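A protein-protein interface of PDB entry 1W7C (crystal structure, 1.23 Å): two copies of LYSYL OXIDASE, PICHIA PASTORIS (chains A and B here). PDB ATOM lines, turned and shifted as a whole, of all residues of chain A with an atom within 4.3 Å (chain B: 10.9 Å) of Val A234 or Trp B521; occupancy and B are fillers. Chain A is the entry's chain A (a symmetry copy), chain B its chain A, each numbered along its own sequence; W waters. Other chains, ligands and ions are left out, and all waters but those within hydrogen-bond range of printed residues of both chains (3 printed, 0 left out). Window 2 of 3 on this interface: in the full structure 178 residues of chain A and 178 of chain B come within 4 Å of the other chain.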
ATOM      1  N   TYR A 190      -5.689  -4.794  15.656  1.00  0.00           N
ATOM      2  CA  TYR A 190      -5.119  -3.593  15.090  1.00  0.00           C
ATOM      3  C   TYR A 190      -5.343  -3.612  13.577  1.00  0.00           C
ATOM      4  O   TYR A 190      -5.725  -4.619  12.997  1.00  0.00           O
ATOM      5  CB  TYR A 190      -3.627  -3.510  15.410  1.00  0.00           C
ATOM      6  CG  TYR A 190      -3.339  -3.194  16.871  1.00  0.00           C
ATOM      7  CD1 TYR A 190      -3.267  -4.202  17.818  1.00  0.00           C
ATOM      8  CD2 TYR A 190      -3.135  -1.891  17.310  1.00  0.00           C
ATOM      9  CE1 TYR A 190      -2.998  -3.922  19.141  1.00  0.00           C
ATOM     10  CE2 TYR A 190      -2.840  -1.600  18.648  1.00  0.00           C
ATOM     11  CZ  TYR A 190      -2.769  -2.623  19.552  1.00  0.00           C
ATOM     12  OH  TYR A 190      -2.473  -2.315  20.862  1.00  0.00           O
ATOM     13  N   GLU A 227      -8.668   3.086  19.453  1.00  0.00           N
ATOM     14  CA  GLU A 227      -7.567   3.996  19.202  1.00  0.00           C
ATOM     15  C   GLU A 227      -7.356   4.255  17.735  1.00  0.00           C
ATOM     16  O   GLU A 227      -7.579   3.367  16.902  1.00  0.00           O
ATOM     17  CB  GLU A 227      -6.251   3.423  19.763  1.00  0.00           C
ATOM     18  CG  GLU A 227      -6.262   3.155  21.243  1.00  0.00           C
ATOM     19  CD  GLU A 227      -5.018   2.435  21.735  1.00  0.00           C
ATOM     20  OE1 GLU A 227      -4.819   2.369  22.976  1.00  0.00           O
ATOM     21  OE2 GLU A 227      -4.234   1.940  20.886  1.00  0.00           O
ATOM     22  N   TYR A 228      -6.925   5.485  17.441  1.00  0.00           N
ATOM     23  CA  TYR A 228      -6.226   5.814  16.201  1.00  0.00           C
ATOM     24  C   TYR A 228      -4.790   6.126  16.555  1.00  0.00           C
ATOM     25  O   TYR A 228      -4.539   6.820  17.532  1.00  0.00           O
ATOM     26  CB  TYR A 228      -6.890   7.012  15.509  1.00  0.00           C
ATOM     27  CG  TYR A 228      -8.273   6.684  15.025  1.00  0.00           C
ATOM     28  CD1 TYR A 228      -9.410   7.211  15.638  1.00  0.00           C
ATOM     29  CD2 TYR A 228      -8.440   5.774  13.986  1.00  0.00           C
ATOM     30  CE1 TYR A 228     -10.675   6.865  15.185  1.00  0.00           C
ATOM     31  CE2 TYR A 228      -9.685   5.416  13.542  1.00  0.00           C
ATOM     32  CZ  TYR A 228     -10.802   5.959  14.136  1.00  0.00           C
ATOM     33  OH  TYR A 228     -12.036   5.583  13.650  1.00  0.00           O
ATOM     34  N   ILE A 229      -3.848   5.618  15.772  1.00  0.00           N
ATOM     35  CA  ILE A 229      -2.434   5.762  16.079  1.00  0.00           C
ATOM     36  C   ILE A 229      -1.744   6.308  14.843  1.00  0.00           C
ATOM     37  O   ILE A 229      -1.867   5.739  13.764  1.00  0.00           O
ATOM     38  CB  ILE A 229      -1.831   4.412  16.501  1.00  0.00           C
ATOM     39  CG1 ILE A 229      -2.517   3.876  17.760  1.00  0.00           C
ATOM     40  CG2 ILE A 229      -0.315   4.523  16.665  1.00  0.00           C
ATOM     41  CD1 ILE A 229      -2.333   2.403  17.975  1.00  0.00           C
ATOM     42  N   ASN A 232       3.272   7.623  16.067  1.00  0.00           N
ATOM     43  CA  ASN A 232       3.503   7.071  17.405  1.00  0.00           C
ATOM     44  C   ASN A 232       2.723   7.734  18.547  1.00  0.00           C
ATOM     45  O   ASN A 232       3.076   7.569  19.701  1.00  0.00           O
ATOM     46  CB  ASN A 232       5.009   7.053  17.721  1.00  0.00           C
ATOM     47  CG  ASN A 232       5.752   6.036  16.897  1.00  0.00           C
ATOM     48  OD1 ASN A 232       5.446   4.833  16.986  1.00  0.00           O
ATOM     49  ND2 ASN A 232       6.704   6.490  16.068  1.00  0.00           N
ATOM     50  N   LYS A 233       1.651   8.429  18.185  1.00  0.00           N
ATOM     51  CA  LYS A 233       0.746   9.060  19.134  1.00  0.00           C
ATOM     52  C   LYS A 233      -0.597   8.341  19.102  1.00  0.00           C
ATOM     53  O   LYS A 233      -1.039   7.909  18.070  1.00  0.00           O
ATOM     54  CB  LYS A 233       0.587  10.546  18.803  1.00  0.00           C
ATOM     55  CG  LYS A 233       1.910  11.303  18.913  1.00  0.00           C
ATOM     56  CD  LYS A 233       1.720  12.811  18.906  1.00  0.00           C
ATOM     57  CE  LYS A 233       3.054  13.560  18.784  1.00  0.00           C
ATOM     58  NZ  LYS A 233       3.866  13.433  20.015  1.00  0.00           N
ATOM     59  N   VAL A 234      -1.203   8.205  20.274  1.00  0.00           N
ATOM     60  CA  VAL A 234      -2.466   7.505  20.459  1.00  0.00           C
ATOM     61  C   VAL A 234      -3.589   8.500  20.699  1.00  0.00           C
ATOM     62  O   VAL A 234      -3.477   9.358  21.584  1.00  0.00           O
ATOM     63  CB  VAL A 234      -2.394   6.533  21.656  1.00  0.00           C
ATOM     64  CG1 VAL A 234      -3.698   5.771  21.818  1.00  0.00           C
ATOM     65  CG2 VAL A 234      -1.210   5.557  21.489  1.00  0.00           C
ATOM     66  N   TYR A 235      -4.673   8.327  19.945  1.00  0.00           N
ATOM     67  CA  TYR A 235      -5.886   9.123  20.070  1.00  0.00           C
ATOM     68  C   TYR A 235      -7.028   8.171  20.401  1.00  0.00           C
ATOM     69  O   TYR A 235      -7.113   7.086  19.839  1.00  0.00           O
ATOM     70  CB  TYR A 235      -6.147   9.884  18.764  1.00  0.00           C
ATOM     71  CG  TYR A 235      -4.983  10.746  18.368  1.00  0.00           C
ATOM     72  CD1 TYR A 235      -3.954  10.241  17.578  1.00  0.00           C
ATOM     73  CD2 TYR A 235      -4.888  12.058  18.804  1.00  0.00           C
ATOM     74  CE1 TYR A 235      -2.854  11.026  17.244  1.00  0.00           C
ATOM     75  CE2 TYR A 235      -3.809  12.846  18.478  1.00  0.00           C
ATOM     76  CZ  TYR A 235      -2.790  12.339  17.692  1.00  0.00           C
ATOM     77  OH  TYR A 235      -1.706  13.144  17.361  1.00  0.00           O
ATOM     78  N   ASP A 347       8.342  -1.306  14.528  1.00  0.00           N
ATOM     79  CA  ASP A 347       7.995  -0.225  15.413  1.00  0.00           C
ATOM     80  C   ASP A 347       6.514   0.077  15.414  1.00  0.00           C
ATOM     81  O   ASP A 347       6.055   0.791  16.312  1.00  0.00           O
ATOM     82  CB  ASP A 347       8.761   1.066  15.055  1.00  0.00           C
ATOM     83  CG  ASP A 347       8.524   1.537  13.605  1.00  0.00           C
ATOM     84  OD1 ASP A 347       8.404   0.678  12.685  1.00  0.00           O
ATOM     85  OD2 ASP A 347       8.514   2.750  13.297  1.00  0.00           O
ATOM     86  N   ASP A 348       5.770  -0.427  14.427  1.00  0.00           N
ATOM     87  CA  ASP A 348       4.375  -0.022  14.220  1.00  0.00           C
ATOM     88  C   ASP A 348       3.402  -1.112  14.619  1.00  0.00           C
ATOM     89  O   ASP A 348       3.772  -2.283  14.689  1.00  0.00           O
ATOM     90  CB  ASP A 348       4.173   0.556  12.798  1.00  0.00           C
ATOM     91  CG  ASP A 348       3.903  -0.461  11.740  1.00  0.00           C
ATOM     92  OD1 ASP A 348       4.432  -0.231  10.611  1.00  0.00           O
ATOM     93  OD2 ASP A 348       3.114  -1.414  11.887  1.00  0.00           O
ATOM     94  N   PRO A 349       2.179  -0.729  14.983  1.00  0.00           N
ATOM     95  CA  PRO A 349       1.240  -1.699  15.552  1.00  0.00           C
ATOM     96  C   PRO A 349       0.528  -2.584  14.523  1.00  0.00           C
ATOM     97  O   PRO A 349      -0.317  -3.407  14.913  1.00  0.00           O
ATOM     98  CB  PRO A 349       0.236  -0.824  16.276  1.00  0.00           C
ATOM     99  CG  PRO A 349       0.227   0.439  15.482  1.00  0.00           C
ATOM    100  CD  PRO A 349       1.643   0.644  15.035  1.00  0.00           C
ATOM    101  N   HIS A 353       2.169  -6.741  15.037  1.00  0.00           N
ATOM    102  CA  HIS A 353       1.098  -7.672  15.348  1.00  0.00           C
ATOM    103  C   HIS A 353       0.797  -8.647  14.216  1.00  0.00           C
ATOM    104  O   HIS A 353      -0.231  -9.302  14.232  1.00  0.00           O
ATOM    105  CB  HIS A 353      -0.160  -6.900  15.757  1.00  0.00           C
ATOM    106  CG  HIS A 353      -0.009  -6.193  17.072  1.00  0.00           C
ATOM    107  ND1 HIS A 353      -0.025  -4.819  17.189  1.00  0.00           N
ATOM    108  CD2 HIS A 353       0.231  -6.680  18.316  1.00  0.00           C
ATOM    109  CE1 HIS A 353       0.164  -4.494  18.460  1.00  0.00           C
ATOM    110  NE2 HIS A 353       0.307  -5.603  19.167  1.00  0.00           N
ATOM    111  N   VAL B 517      11.020  -4.794  24.355  1.00  0.00           N
ATOM    112  CA  VAL B 517      10.781  -3.372  24.131  1.00  0.00           C
ATOM    113  C   VAL B 517       9.403  -2.985  24.624  1.00  0.00           C
ATOM    114  O   VAL B 517       8.538  -3.823  24.837  1.00  0.00           O
ATOM    115  CB  VAL B 517      10.883  -2.965  22.642  1.00  0.00           C
ATOM    116  CG1 VAL B 517      12.220  -3.358  22.030  1.00  0.00           C
ATOM    117  CG2 VAL B 517       9.749  -3.528  21.825  1.00  0.00           C
ATOM    118  N   GLU B 518       9.237  -1.692  24.849  1.00  0.00           N
ATOM    119  CA  GLU B 518       7.953  -1.091  25.075  1.00  0.00           C
ATOM    120  C   GLU B 518       7.789  -0.076  23.967  1.00  0.00           C
ATOM    121  O   GLU B 518       8.752   0.611  23.606  1.00  0.00           O
ATOM    122  CB  GLU B 518       7.905  -0.388  26.431  1.00  0.00           C
ATOM    123  CG  GLU B 518       7.961  -1.329  27.628  1.00  0.00           C
ATOM    124  CD  GLU B 518       7.740  -0.634  28.971  1.00  0.00           C
ATOM    125  OE1 GLU B 518       7.207   0.503  29.004  1.00  0.00           O
ATOM    126  OE2 GLU B 518       8.100  -1.235  30.012  1.00  0.00           O
ATOM    127  N   TYR B 519       6.583   0.014  23.411  1.00  0.00           N
ATOM    128  CA  TYR B 519       6.279   0.954  22.343  1.00  0.00           C
ATOM    129  C   TYR B 519       5.478   2.137  22.858  1.00  0.00           C
ATOM    130  O   TYR B 519       4.689   1.988  23.807  1.00  0.00           O
ATOM    131  CB  TYR B 519       5.440   0.275  21.271  1.00  0.00           C
ATOM    132  CG  TYR B 519       6.137  -0.873  20.566  1.00  0.00           C
ATOM    133  CD1 TYR B 519       5.804  -2.206  20.851  1.00  0.00           C
ATOM    134  CD2 TYR B 519       7.091  -0.636  19.593  1.00  0.00           C
ATOM    135  CE1 TYR B 519       6.438  -3.233  20.241  1.00  0.00           C
ATOM    136  CE2 TYR B 519       7.750  -1.675  18.962  1.00  0.00           C
ATOM    137  CZ  TYR B 519       7.408  -2.974  19.293  1.00  0.00           C
ATOM    138  OH  TYR B 519       7.992  -4.030  18.633  1.00  0.00           O
ATOM    139  N   PRO B 520       5.653   3.308  22.240  1.00  0.00           N
ATOM    140  CA  PRO B 520       4.914   4.504  22.669  1.00  0.00           C
ATOM    141  C   PRO B 520       3.401   4.373  22.525  1.00  0.00           C
ATOM    142  O   PRO B 520       2.658   5.026  23.275  1.00  0.00           O
ATOM    143  CB  PRO B 520       5.465   5.607  21.751  1.00  0.00           C
ATOM    144  CG  PRO B 520       6.075   4.903  20.595  1.00  0.00           C
ATOM    145  CD  PRO B 520       6.581   3.603  21.127  1.00  0.00           C
ATOM    146  N   TRP B 521       2.958   3.503  21.620  1.00  0.00           N
ATOM    147  CA  TRP B 521       1.534   3.302  21.391  1.00  0.00           C
ATOM    148  C   TRP B 521       0.907   2.246  22.303  1.00  0.00           C
ATOM    149  O   TRP B 521      -0.307   2.023  22.249  1.00  0.00           O
ATOM    150  CB  TRP B 521       1.255   3.001  19.917  1.00  0.00           C
ATOM    151  CG  TRP B 521       2.193   2.005  19.253  1.00  0.00           C
ATOM    152  CD1 TRP B 521       3.205   2.281  18.380  1.00  0.00           C
ATOM    153  CD2 TRP B 521       2.169   0.581  19.402  1.00  0.00           C
ATOM    154  NE1 TRP B 521       3.799   1.112  17.964  1.00  0.00           N
ATOM    155  CE2 TRP B 521       3.188   0.056  18.580  1.00  0.00           C
ATOM    156  CE3 TRP B 521       1.370  -0.306  20.129  1.00  0.00           C
ATOM    157  CZ2 TRP B 521       3.455  -1.305  18.504  1.00  0.00           C
ATOM    158  CZ3 TRP B 521       1.621  -1.655  20.039  1.00  0.00           C
ATOM    159  CH2 TRP B 521       2.667  -2.139  19.255  1.00  0.00           C
ATOM    160  N   ALA B 522       1.704   1.595  23.140  1.00  0.00           N
ATOM    161  CA  ALA B 522       1.142   0.737  24.179  1.00  0.00           C
ATOM    162  C   ALA B 522       1.957   0.847  25.458  1.00  0.00           C
ATOM    163  O   ALA B 522       2.694  -0.064  25.809  1.00  0.00           O
ATOM    164  CB  ALA B 522       1.054  -0.713  23.710  1.00  0.00           C
ATOM    165  N   PRO B 523       1.848   1.974  26.163  1.00  0.00           N
ATOM    166  CA  PRO B 523       2.717   2.212  27.318  1.00  0.00           C
ATOM    167  C   PRO B 523       2.566   1.121  28.371  1.00  0.00           C
ATOM    168  O   PRO B 523       1.444   0.706  28.677  1.00  0.00           O
ATOM    169  CB  PRO B 523       2.230   3.562  27.869  1.00  0.00           C
ATOM    170  CG  PRO B 523       1.492   4.200  26.731  1.00  0.00           C
ATOM    171  CD  PRO B 523       0.917   3.093  25.928  1.00  0.00           C
ATOM    172  N   GLY B 524       3.690   0.631  28.874  1.00  0.00           N
ATOM    173  CA  GLY B 524       3.703  -0.322  29.964  1.00  0.00           C
ATOM    174  C   GLY B 524       3.666  -1.785  29.531  1.00  0.00           C
ATOM    175  O   GLY B 524       3.856  -2.668  30.359  1.00  0.00           O
ATOM    176  N   THR B 525       3.417  -2.049  28.247  1.00  0.00           N
ATOM    177  CA  THR B 525       3.298  -3.415  27.756  1.00  0.00           C
ATOM    178  C   THR B 525       4.627  -3.825  27.113  1.00  0.00           C
ATOM    179  O   THR B 525       5.054  -3.249  26.100  1.00  0.00           O
ATOM    180  CB  THR B 525       2.134  -3.520  26.720  1.00  0.00           C
ATOM    181  OG1 THR B 525       0.891  -3.178  27.337  1.00  0.00           O
ATOM    182  CG2 THR B 525       1.891  -4.958  26.236  1.00  0.00           C
ATOM    183  N   VAL B 526       5.277  -4.835  27.689  1.00  0.00           N
ATOM    184  CA  VAL B 526       6.547  -5.335  27.156  1.00  0.00           C
ATOM    185  C   VAL B 526       6.281  -6.354  26.067  1.00  0.00           C
ATOM    186  O   VAL B 526       5.449  -7.242  26.234  1.00  0.00           O
ATOM    187  CB  VAL B 526       7.419  -5.967  28.239  1.00  0.00           C
ATOM    188  CG1 VAL B 526       8.703  -6.477  27.655  1.00  0.00           C
ATOM    189  CG2 VAL B 526       7.722  -4.940  29.283  1.00  0.00           C
ATOM    190  N   TYR B 527       6.958  -6.177  24.941  1.00  0.00           N
ATOM    191  CA  TYR B 527       6.909  -7.098  23.805  1.00  0.00           C
ATOM    192  C   TYR B 527       8.307  -7.675  23.616  1.00  0.00           C
ATOM    193  O   TYR B 527       9.300  -6.950  23.649  1.00  0.00           O
ATOM    194  CB  TYR B 527       6.556  -6.357  22.508  1.00  0.00           C
ATOM    195  CG  TYR B 527       5.083  -6.025  22.302  1.00  0.00           C
ATOM    196  CD1 TYR B 527       4.472  -5.014  23.025  1.00  0.00           C
ATOM    197  CD2 TYR B 527       4.316  -6.705  21.373  1.00  0.00           C
ATOM    198  CE1 TYR B 527       3.122  -4.701  22.808  1.00  0.00           C
ATOM    199  CE2 TYR B 527       2.966  -6.397  21.156  1.00  0.00           C
ATOM    200  CZ  TYR B 527       2.390  -5.377  21.850  1.00  0.00           C
ATOM    201  OH  TYR B 527       1.071  -5.083  21.655  1.00  0.00           O
ATOM    202  N   ASN B 528       8.373  -8.968  23.358  1.00  0.00           N
ATOM    203  CA  ASN B 528       9.575  -9.598  22.854  1.00  0.00           C
ATOM    204  C   ASN B 528       9.480  -9.577  21.330  1.00  0.00           C
ATOM    205  O   ASN B 528       8.595 -10.201  20.755  1.00  0.00           O
ATOM    206  CB  ASN B 528       9.678 -11.029  23.366  1.00  0.00           C
ATOM    207  CG  ASN B 528      10.947 -11.730  22.924  1.00  0.00           C
ATOM    208  OD1 ASN B 528      10.867 -12.821  22.417  1.00  0.00           O
ATOM    209  ND2 ASN B 528      12.123 -11.163  23.246  1.00  0.00           N
ATOM    210  N   THR B 529      10.344  -8.799  20.715  1.00  0.00           N
ATOM    211  CA  THR B 529      10.380  -8.623  19.282  1.00  0.00           C
ATOM    212  C   THR B 529      11.778  -8.892  18.773  1.00  0.00           C
ATOM    213  O   THR B 529      12.586  -9.501  19.479  1.00  0.00           O
ATOM    214  CB  THR B 529       9.799  -7.255  18.897  1.00  0.00           C
ATOM    215  OG1 THR B 529       9.659  -7.145  17.469  1.00  0.00           O
ATOM    216  CG2 THR B 529      10.676  -6.103  19.407  1.00  0.00           C
HETATM  217  O   HOH W   1      -2.359   0.238  21.558  1.00  0.00           O
HETATM  218  O   HOH W   2      -2.398   2.757  23.999  1.00  0.00           O
HETATM  219  O   HOH W   3      -0.964  -3.701  22.798  1.00  0.00           O
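Among the printed residues, merely in contact across the chains: His A353 with Trp B521, Val A234 with Trp B521, Asn A232 with Pro B520, Pro A349 with Trp B521, Asn A232 with Trp B521, Asp A347 with Tyr B519, Asp A348 with Trp B521 and Ile A229 with Trp B521.
N of Tyr B527 lies within hydrogen-bond range of O of Val B517. O of Pro A349 sits at hydrogen-bond distance from ND1 of His A353, at 2.7 Å.
NE1 of Trp B521 lies within hydrogen-bond range of O of Asp A347 (2.8 Å). A ring nitrogen (NE2) of His A353 lies within hydrogen-bond range of the side-chain hydroxyl (OH) of Tyr B527, at 2.7 Å.
Val A234 touches just one residue of chain B: Trp B521. Of the printed residues of chain A, Trp B521 touches Ile A229, Asn A232, Val A234, Asp A347, Asp A348, Pro A349 and His A353. No residue of chain B comes within 4 Å of Glu A227. Asn A232 touches just these residues of chain B: Pro B520 (3.7 Å) and Trp B521 (3.7 Å). No residue of chain B comes within 4 Å of Tyr A235. Of chain B, only Trp B521 comes within 4 Å of Pro A349. Printed residues of chain B within 4 Å of Asp A348: Trp B521. Printed residues of chain B within 4 Å of Asp A347: Tyr B519 (3.7 Å) and Trp B521 (2.8 Å). Printed residues of chain A within 4 Å of Pro B520: Asn A232. Printed residues of chain B within 4 Å of Ile A229: Trp B521. Of the printed residues of chain A, Tyr B527 touches His A353 (2.7 Å). The nearest printed residue of chain B that does not touch Asp A347 is Pro B520 (5.6 Å).
No position is printed for both chains. Of the 10 pairs that touch across the chains among the printed residues, none has its exchanged pair printed and touching as well.
Printed residues of chain B that touch a printed residue of chain A: Tyr B519, Pro B520, Trp B521 and Tyr B527. Of the 12 printed residues of chain A, 7 touch a printed residue of chain B. Among the printed residues, 10 pairs touch across the chains. Among the printed residues, no Asp or Glu carboxylate lies within 4 Å of a Lys or Arg side-chain nitrogen of the other chain.
Water W1 lies within hydrogen-bond range of the side-chain carboxylate of Glu A227 (2.6 Å), the side-chain hydroxyl of Tyr A190 (2.6 Å) and the backbone carbonyl oxygen of Trp B521 (2.8 Å). Water W2 bridges OE1 of Glu A227 and O of Trp B521. Water W3 lies within hydrogen-bond range of OH of Tyr B527 (2.7 Å) and OH of Tyr A190 (2.8 Å).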
